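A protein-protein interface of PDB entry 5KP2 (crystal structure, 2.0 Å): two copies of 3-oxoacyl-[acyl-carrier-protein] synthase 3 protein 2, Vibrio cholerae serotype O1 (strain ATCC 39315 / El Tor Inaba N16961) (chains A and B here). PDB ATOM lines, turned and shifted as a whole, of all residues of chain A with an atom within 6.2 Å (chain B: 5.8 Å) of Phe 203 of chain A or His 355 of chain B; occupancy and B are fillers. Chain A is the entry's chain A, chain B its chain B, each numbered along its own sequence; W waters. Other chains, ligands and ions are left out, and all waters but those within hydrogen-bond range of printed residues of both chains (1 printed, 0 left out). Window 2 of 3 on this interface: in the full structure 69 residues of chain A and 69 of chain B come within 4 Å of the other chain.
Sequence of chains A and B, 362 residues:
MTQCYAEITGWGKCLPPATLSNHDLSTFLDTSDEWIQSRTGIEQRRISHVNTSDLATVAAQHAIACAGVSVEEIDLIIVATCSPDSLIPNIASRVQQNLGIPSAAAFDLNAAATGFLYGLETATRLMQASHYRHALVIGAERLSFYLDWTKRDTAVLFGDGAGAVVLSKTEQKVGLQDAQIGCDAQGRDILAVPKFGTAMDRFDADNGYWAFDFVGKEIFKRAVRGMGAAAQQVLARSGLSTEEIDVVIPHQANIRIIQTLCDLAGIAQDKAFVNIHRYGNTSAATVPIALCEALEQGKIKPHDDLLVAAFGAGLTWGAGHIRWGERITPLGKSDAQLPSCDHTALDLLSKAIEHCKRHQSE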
ATOM      1  N   MET A 200      -1.688  -3.773  18.016  1.00  0.00           N
ATOM      2  CA  MET A 200      -2.335  -3.846  16.700  1.00  0.00           C
ATOM      3  C   MET A 200      -1.720  -4.935  15.813  1.00  0.00           C
ATOM      4  O   MET A 200      -0.565  -5.322  16.005  1.00  0.00           O
ATOM      5  CB  MET A 200      -2.280  -2.476  15.984  1.00  0.00           C
ATOM      6  CG  MET A 200      -0.977  -2.142  15.261  1.00  0.00           C
ATOM      7  SD  MET A 200      -0.752  -0.369  14.949  1.00  0.00           S
ATOM      8  CE  MET A 200      -2.154  -0.037  13.876  1.00  0.00           C
ATOM      9  N   ASP A 201      -2.505  -5.425  14.851  1.00  0.00           N
ATOM     10  CA  ASP A 201      -2.006  -6.343  13.827  1.00  0.00           C
ATOM     11  C   ASP A 201      -1.274  -5.541  12.742  1.00  0.00           C
ATOM     12  O   ASP A 201      -1.896  -4.887  11.905  1.00  0.00           O
ATOM     13  CB  ASP A 201      -3.137  -7.179  13.227  1.00  0.00           C
ATOM     14  CG  ASP A 201      -2.626  -8.360  12.392  1.00  0.00           C
ATOM     15  OD1 ASP A 201      -1.459  -8.349  11.937  1.00  0.00           O
ATOM     16  OD2 ASP A 201      -3.402  -9.314  12.169  1.00  0.00           O
ATOM     17  N   ARG A 202       0.052  -5.632  12.770  1.00  0.00           N
ATOM     18  CA  ARG A 202       0.941  -4.890  11.869  1.00  0.00           C
ATOM     19  C   ARG A 202       0.697  -5.141  10.373  1.00  0.00           C
ATOM     20  O   ARG A 202       0.912  -4.244   9.565  1.00  0.00           O
ATOM     21  CB  ARG A 202       2.397  -5.236  12.201  1.00  0.00           C
ATOM     22  CG  ARG A 202       3.451  -4.516  11.378  1.00  0.00           C
ATOM     23  CD  ARG A 202       4.838  -4.921  11.838  1.00  0.00           C
ATOM     24  NE  ARG A 202       5.860  -4.624  10.847  1.00  0.00           N
ATOM     25  CZ  ARG A 202       7.119  -5.055  10.895  1.00  0.00           C
ATOM     26  NH1 ARG A 202       7.556  -5.808  11.905  1.00  0.00           N
ATOM     27  NH2 ARG A 202       7.957  -4.726   9.919  1.00  0.00           N
ATOM     28  N   PHE A 203       0.275  -6.352  10.015  1.00  0.00           N
ATOM     29  CA  PHE A 203       0.125  -6.748   8.609  1.00  0.00           C
ATOM     30  C   PHE A 203      -1.320  -6.877   8.125  1.00  0.00           C
ATOM     31  O   PHE A 203      -1.556  -7.314   7.001  1.00  0.00           O
ATOM     32  CB  PHE A 203       0.912  -8.039   8.357  1.00  0.00           C
ATOM     33  CG  PHE A 203       2.377  -7.904   8.658  1.00  0.00           C
ATOM     34  CD1 PHE A 203       3.192  -7.121   7.841  1.00  0.00           C
ATOM     35  CD2 PHE A 203       2.940  -8.524   9.766  1.00  0.00           C
ATOM     36  CE1 PHE A 203       4.543  -6.974   8.116  1.00  0.00           C
ATOM     37  CE2 PHE A 203       4.294  -8.378  10.049  1.00  0.00           C
ATOM     38  CZ  PHE A 203       5.096  -7.607   9.219  1.00  0.00           C
ATOM     39  N   ASP A 204      -2.277  -6.500   8.965  1.00  0.00           N
ATOM     40  CA  ASP A 204      -3.687  -6.470   8.582  1.00  0.00           C
ATOM     41  C   ASP A 204      -3.926  -5.184   7.806  1.00  0.00           C
ATOM     42  O   ASP A 204      -3.675  -4.096   8.323  1.00  0.00           O
ATOM     43  CB  ASP A 204      -4.569  -6.526   9.836  1.00  0.00           C
ATOM     44  CG  ASP A 204      -6.067  -6.480   9.531  1.00  0.00           C
ATOM     45  OD1 ASP A 204      -6.487  -6.570   8.357  1.00  0.00           O
ATOM     46  OD2 ASP A 204      -6.836  -6.343  10.503  1.00  0.00           O
ATOM     47  N   ALA A 205      -4.412  -5.315   6.571  1.00  0.00           N
ATOM     48  CA  ALA A 205      -4.690  -4.159   5.700  1.00  0.00           C
ATOM     49  C   ALA A 205      -5.780  -3.211   6.247  1.00  0.00           C
ATOM     50  O   ALA A 205      -5.805  -2.035   5.889  1.00  0.00           O
ATOM     51  CB  ALA A 205      -5.050  -4.628   4.295  1.00  0.00           C
ATOM     52  N   ASN A 207      -6.061  -2.535   9.569  1.00  0.00           N
ATOM     53  CA  ASN A 207      -5.643  -2.102  10.916  1.00  0.00           C
ATOM     54  C   ASN A 207      -5.794  -0.591  11.195  1.00  0.00           C
ATOM     55  O   ASN A 207      -5.767  -0.174  12.344  1.00  0.00           O
ATOM     56  CB  ASN A 207      -4.221  -2.605  11.264  1.00  0.00           C
ATOM     57  CG  ASN A 207      -3.124  -1.962  10.430  1.00  0.00           C
ATOM     58  OD1 ASN A 207      -3.358  -1.039   9.655  1.00  0.00           O
ATOM     59  ND2 ASN A 207      -1.906  -2.465  10.588  1.00  0.00           N
ATOM     60  N   LEU B 147      10.449  -5.837  13.944  1.00  0.00           N
ATOM     61  CA  LEU B 147      11.564  -6.343  13.137  1.00  0.00           C
ATOM     62  C   LEU B 147      11.170  -6.687  11.699  1.00  0.00           C
ATOM     63  O   LEU B 147      10.036  -7.087  11.438  1.00  0.00           O
ATOM     64  CB  LEU B 147      12.225  -7.556  13.830  1.00  0.00           C
ATOM     65  CG  LEU B 147      12.761  -7.330  15.255  1.00  0.00           C
ATOM     66  CD1 LEU B 147      13.367  -8.605  15.832  1.00  0.00           C
ATOM     67  CD2 LEU B 147      13.799  -6.212  15.282  1.00  0.00           C
ATOM     68  N   TRP B 149      11.910  -9.378   9.139  1.00  0.00           N
ATOM     69  CA  TRP B 149      12.412 -10.760   9.218  1.00  0.00           C
ATOM     70  C   TRP B 149      13.159 -11.252   7.966  1.00  0.00           C
ATOM     71  O   TRP B 149      13.628 -12.389   7.936  1.00  0.00           O
ATOM     72  CB  TRP B 149      11.265 -11.708   9.588  1.00  0.00           C
ATOM     73  CG  TRP B 149      10.693 -11.369  10.938  1.00  0.00           C
ATOM     74  CD1 TRP B 149       9.497 -10.754  11.198  1.00  0.00           C
ATOM     75  CD2 TRP B 149      11.323 -11.566  12.201  1.00  0.00           C
ATOM     76  NE1 TRP B 149       9.333 -10.578  12.553  1.00  0.00           N
ATOM     77  CE2 TRP B 149      10.444 -11.065  13.192  1.00  0.00           C
ATOM     78  CE3 TRP B 149      12.537 -12.143  12.599  1.00  0.00           C
ATOM     79  CZ2 TRP B 149      10.751 -11.113  14.553  1.00  0.00           C
ATOM     80  CZ3 TRP B 149      12.845 -12.197  13.952  1.00  0.00           C
ATOM     81  CH2 TRP B 149      11.954 -11.687  14.914  1.00  0.00           C
ATOM     82  N   ALA B 205      -2.067   0.370   2.885  1.00  0.00           N
ATOM     83  CA  ALA B 205      -2.065  -1.077   3.174  1.00  0.00           C
ATOM     84  C   ALA B 205      -0.654  -1.680   3.384  1.00  0.00           C
ATOM     85  O   ALA B 205      -0.519  -2.704   4.040  1.00  0.00           O
ATOM     86  CB  ALA B 205      -2.807  -1.836   2.077  1.00  0.00           C
ATOM     87  N   GLY B 208       2.858  -1.331   7.199  1.00  0.00           N
ATOM     88  CA  GLY B 208       3.580  -2.261   8.059  1.00  0.00           C
ATOM     89  C   GLY B 208       5.022  -2.579   7.663  1.00  0.00           C
ATOM     90  O   GLY B 208       5.790  -3.051   8.500  1.00  0.00           O
ATOM     91  N   TYR B 209       5.391  -2.335   6.402  1.00  0.00           N
ATOM     92  CA  TYR B 209       6.719  -2.694   5.893  1.00  0.00           C
ATOM     93  C   TYR B 209       7.659  -1.492   5.985  1.00  0.00           C
ATOM     94  O   TYR B 209       8.104  -0.946   4.976  1.00  0.00           O
ATOM     95  CB  TYR B 209       6.605  -3.243   4.465  1.00  0.00           C
ATOM     96  CG  TYR B 209       5.661  -4.421   4.386  1.00  0.00           C
ATOM     97  CD1 TYR B 209       6.074  -5.699   4.765  1.00  0.00           C
ATOM     98  CD2 TYR B 209       4.333  -4.250   3.966  1.00  0.00           C
ATOM     99  CE1 TYR B 209       5.195  -6.774   4.712  1.00  0.00           C
ATOM    100  CE2 TYR B 209       3.449  -5.322   3.908  1.00  0.00           C
ATOM    101  CZ  TYR B 209       3.883  -6.578   4.285  1.00  0.00           C
ATOM    102  OH  TYR B 209       3.011  -7.640   4.215  1.00  0.00           O
ATOM    103  N   SER B 350       5.540 -16.800  12.628  1.00  0.00           N
ATOM    104  CA  SER B 350       5.152 -17.389  11.334  1.00  0.00           C
ATOM    105  C   SER B 350       4.474 -16.424  10.357  1.00  0.00           C
ATOM    106  O   SER B 350       4.899 -16.283   9.206  1.00  0.00           O
ATOM    107  CB  SER B 350       4.222 -18.585  11.586  1.00  0.00           C
ATOM    108  OG  SER B 350       3.831 -19.193  10.374  1.00  0.00           O
ATOM    109  N   LYS B 351       3.422 -15.768  10.829  1.00  0.00           N
ATOM    110  CA  LYS B 351       2.675 -14.791  10.027  1.00  0.00           C
ATOM    111  C   LYS B 351       3.566 -13.629   9.560  1.00  0.00           C
ATOM    112  O   LYS B 351       3.577 -13.290   8.379  1.00  0.00           O
ATOM    113  CB  LYS B 351       1.475 -14.255  10.828  1.00  0.00           C
ATOM    114  CG  LYS B 351       0.724 -13.113  10.146  1.00  0.00           C
ATOM    115  CD  LYS B 351      -0.622 -12.796  10.786  1.00  0.00           C
ATOM    116  CE  LYS B 351      -1.442 -11.902   9.869  1.00  0.00           C
ATOM    117  NZ  LYS B 351      -2.714 -11.447  10.493  1.00  0.00           N
ATOM    118  N   ALA B 352       4.308 -13.043  10.498  1.00  0.00           N
ATOM    119  CA  ALA B 352       5.184 -11.904  10.216  1.00  0.00           C
ATOM    120  C   ALA B 352       6.330 -12.250   9.248  1.00  0.00           C
ATOM    121  O   ALA B 352       6.651 -11.459   8.367  1.00  0.00           O
ATOM    122  CB  ALA B 352       5.742 -11.340  11.518  1.00  0.00           C
ATOM    123  N   ILE B 353       6.921 -13.436   9.415  1.00  0.00           N
ATOM    124  CA  ILE B 353       7.965 -13.943   8.514  1.00  0.00           C
ATOM    125  C   ILE B 353       7.418 -14.103   7.079  1.00  0.00           C
ATOM    126  O   ILE B 353       8.019 -13.604   6.111  1.00  0.00           O
ATOM    127  CB  ILE B 353       8.576 -15.275   9.052  1.00  0.00           C
ATOM    128  CG1 ILE B 353       9.401 -15.013  10.322  1.00  0.00           C
ATOM    129  CG2 ILE B 353       9.446 -15.967   8.007  1.00  0.00           C
ATOM    130  CD1 ILE B 353       9.641 -16.244  11.189  1.00  0.00           C
ATOM    131  N   GLU B 354       6.282 -14.782   6.946  1.00  0.00           N
ATOM    132  CA  GLU B 354       5.643 -14.969   5.641  1.00  0.00           C
ATOM    133  C   GLU B 354       5.287 -13.639   4.946  1.00  0.00           C
ATOM    134  O   GLU B 354       5.525 -13.478   3.743  1.00  0.00           O
ATOM    135  CB  GLU B 354       4.386 -15.834   5.778  1.00  0.00           C
ATOM    136  N   HIS B 355       4.708 -12.704   5.695  1.00  0.00           N
ATOM    137  CA  HIS B 355       4.381 -11.380   5.140  1.00  0.00           C
ATOM    138  C   HIS B 355       5.603 -10.623   4.636  1.00  0.00           C
ATOM    139  O   HIS B 355       5.575 -10.076   3.538  1.00  0.00           O
ATOM    140  CB  HIS B 355       3.625 -10.514   6.157  1.00  0.00           C
ATOM    141  CG  HIS B 355       2.158 -10.805   6.217  1.00  0.00           C
ATOM    142  ND1 HIS B 355       1.299 -10.481   5.192  1.00  0.00           N
ATOM    143  CD2 HIS B 355       1.397 -11.372   7.180  1.00  0.00           C
ATOM    144  CE1 HIS B 355       0.072 -10.846   5.516  1.00  0.00           C
ATOM    145  NE2 HIS B 355       0.104 -11.391   6.718  1.00  0.00           N
ATOM    146  N   CYS B 356       6.658 -10.581   5.443  1.00  0.00           N
ATOM    147  CA  CYS B 356       7.891  -9.865   5.071  1.00  0.00           C
ATOM    148  C   CYS B 356       8.526 -10.483   3.825  1.00  0.00           C
ATOM    149  O   CYS B 356       8.942  -9.748   2.920  1.00  0.00           O
ATOM    150  CB  CYS B 356       8.897  -9.829   6.235  1.00  0.00           C
ATOM    151  SG  CYS B 356       8.458  -8.737   7.624  1.00  0.00           S
ATOM    152  N   LYS B 357       8.576 -11.821   3.778  1.00  0.00           N
ATOM    153  CA  LYS B 357       9.063 -12.561   2.591  1.00  0.00           C
ATOM    154  C   LYS B 357       8.243 -12.303   1.301  1.00  0.00           C
ATOM    155  O   LYS B 357       8.810 -12.063   0.225  1.00  0.00           O
ATOM    156  CB  LYS B 357       9.151 -14.071   2.885  1.00  0.00           C
ATOM    157  CG  LYS B 357      10.331 -14.443   3.769  1.00  0.00           C
ATOM    158  CD  LYS B 357      10.213 -15.885   4.240  1.00  0.00           C
ATOM    159  CE  LYS B 357      11.372 -16.281   5.125  1.00  0.00           C
ATOM    160  NZ  LYS B 357      12.598 -16.560   4.329  1.00  0.00           N
ATOM    161  N   ARG B 358       6.919 -12.330   1.426  1.00  0.00           N
ATOM    162  CA  ARG B 358       6.025 -12.051   0.290  1.00  0.00           C
ATOM    163  C   ARG B 358       6.232 -10.634  -0.257  1.00  0.00           C
ATOM    164  O   ARG B 358       6.334 -10.451  -1.471  1.00  0.00           O
ATOM    165  CB  ARG B 358       4.552 -12.249   0.676  1.00  0.00           C
ATOM    166  N   HIS B 359       6.319  -9.653   0.642  1.00  0.00           N
ATOM    167  CA  HIS B 359       6.524  -8.260   0.254  1.00  0.00           C
ATOM    168  C   HIS B 359       7.961  -8.051  -0.212  1.00  0.00           C
ATOM    169  O   HIS B 359       8.187  -7.575  -1.321  1.00  0.00           O
ATOM    170  CB  HIS B 359       6.191  -7.323   1.419  1.00  0.00           C
ATOM    171  CG  HIS B 359       6.317  -5.870   1.084  1.00  0.00           C
ATOM    172  ND1 HIS B 359       7.502  -5.176   1.222  1.00  0.00           N
ATOM    173  CD2 HIS B 359       5.407  -4.975   0.627  1.00  0.00           C
ATOM    174  CE1 HIS B 359       7.316  -3.917   0.864  1.00  0.00           C
ATOM    175  NE2 HIS B 359       6.056  -3.769   0.493  1.00  0.00           N
HETATM  176  O   HOH W   1       1.091  -3.434   6.288  1.00  0.00           O
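NE of Arg 202 of chain A is in hydrogen-bond range of O of Gly 208 of chain B (2.8 Å). OD2 of Asp 201 of chain A is in salt-bridge range of NZ of Lys 351 of chain B (2.8 Å). The guanidinium group (NH1) of Arg 202 of chain A sits at hydrogen-bond distance from the backbone carbonyl oxygen (O) of Leu 147 of chain B (2.8 Å).
Water W1 lies within hydrogen-bond range of O of Ala 205 of chain B, N of Gly 208 of chain B and O of Arg 202 of chain A.
Position printed for both chains: 205. Of the 7 pairs that touch across the chains among the printed residues, none has its exchanged pair printed and touching as well.
Among the printed residues, merely in contact across the chains: Phe 203 of chain A with Tyr 209 of chain B (3.5 Å), Phe 203 of chain A with Ala 352 of chain B (3.6 Å), Phe 203 of chain A with His 355 of chain B (3.6 Å) and Phe 203 of chain A with Cys 356 of chain B (3.9 Å).
O of Arg 202 of chain A sits at hydrogen-bond distance from ND2 of Asn 207 of chain A, 3.5 Å away. ND1 of His 355 of chain B sits at hydrogen-bond distance from OH of Tyr 209 of chain B (3.5 Å). The side-chain sulfur (SG) of Cys 356 of chain B sits at hydrogen-bond distance from the backbone carbonyl oxygen (O) of Ala 352 of chain B (3.4 Å). The side-chain amide nitrogen of Asn 207 of chain A lies within hydrogen-bond range of the backbone carbonyl oxygen of Asp 201 of chain A (2.8 Å). N of Phe 203 of chain A sits close to OD1 of Asp 201 of chain A (3.3 Å).
Phe 203 of chain A touches just these residues of chain B: Tyr 209, Ala 352, His 355 and Cys 356. Of the printed residues of chain A, His 355 of chain B touches Phe 203 (3.6 Å). Printed residues of chain A within 4 Å of Gly 208 of chain B: Arg 202. Of the printed residues of chain B, Arg 202 of chain A touches Leu 147 and Gly 208. Of the printed residues of chain A, Cys 356 of chain B touches Phe 203. Printed residues of chain A within 4 Å of Lys 351 of chain B: Asp 201 (2.8 Å). Of the printed residues of chain A, Leu 147 of chain B touches Arg 202. The nearest residue of chain B that does not touch Phe 203 of chain A is Gly 208 of chain B (4.1 Å). The nearest residue of chain A that does not touch His 355 of chain B is Asp 204 of chain A (5.9 Å).
Among the printed residues, 7 pairs touch across the chains. Among the printed residues, Asp or Glu carboxylates within 4 Å of a Lys or Arg side-chain nitrogen of the other chain: Asp 201 of chain A with Lys 351 of chain B (2.8 Å).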
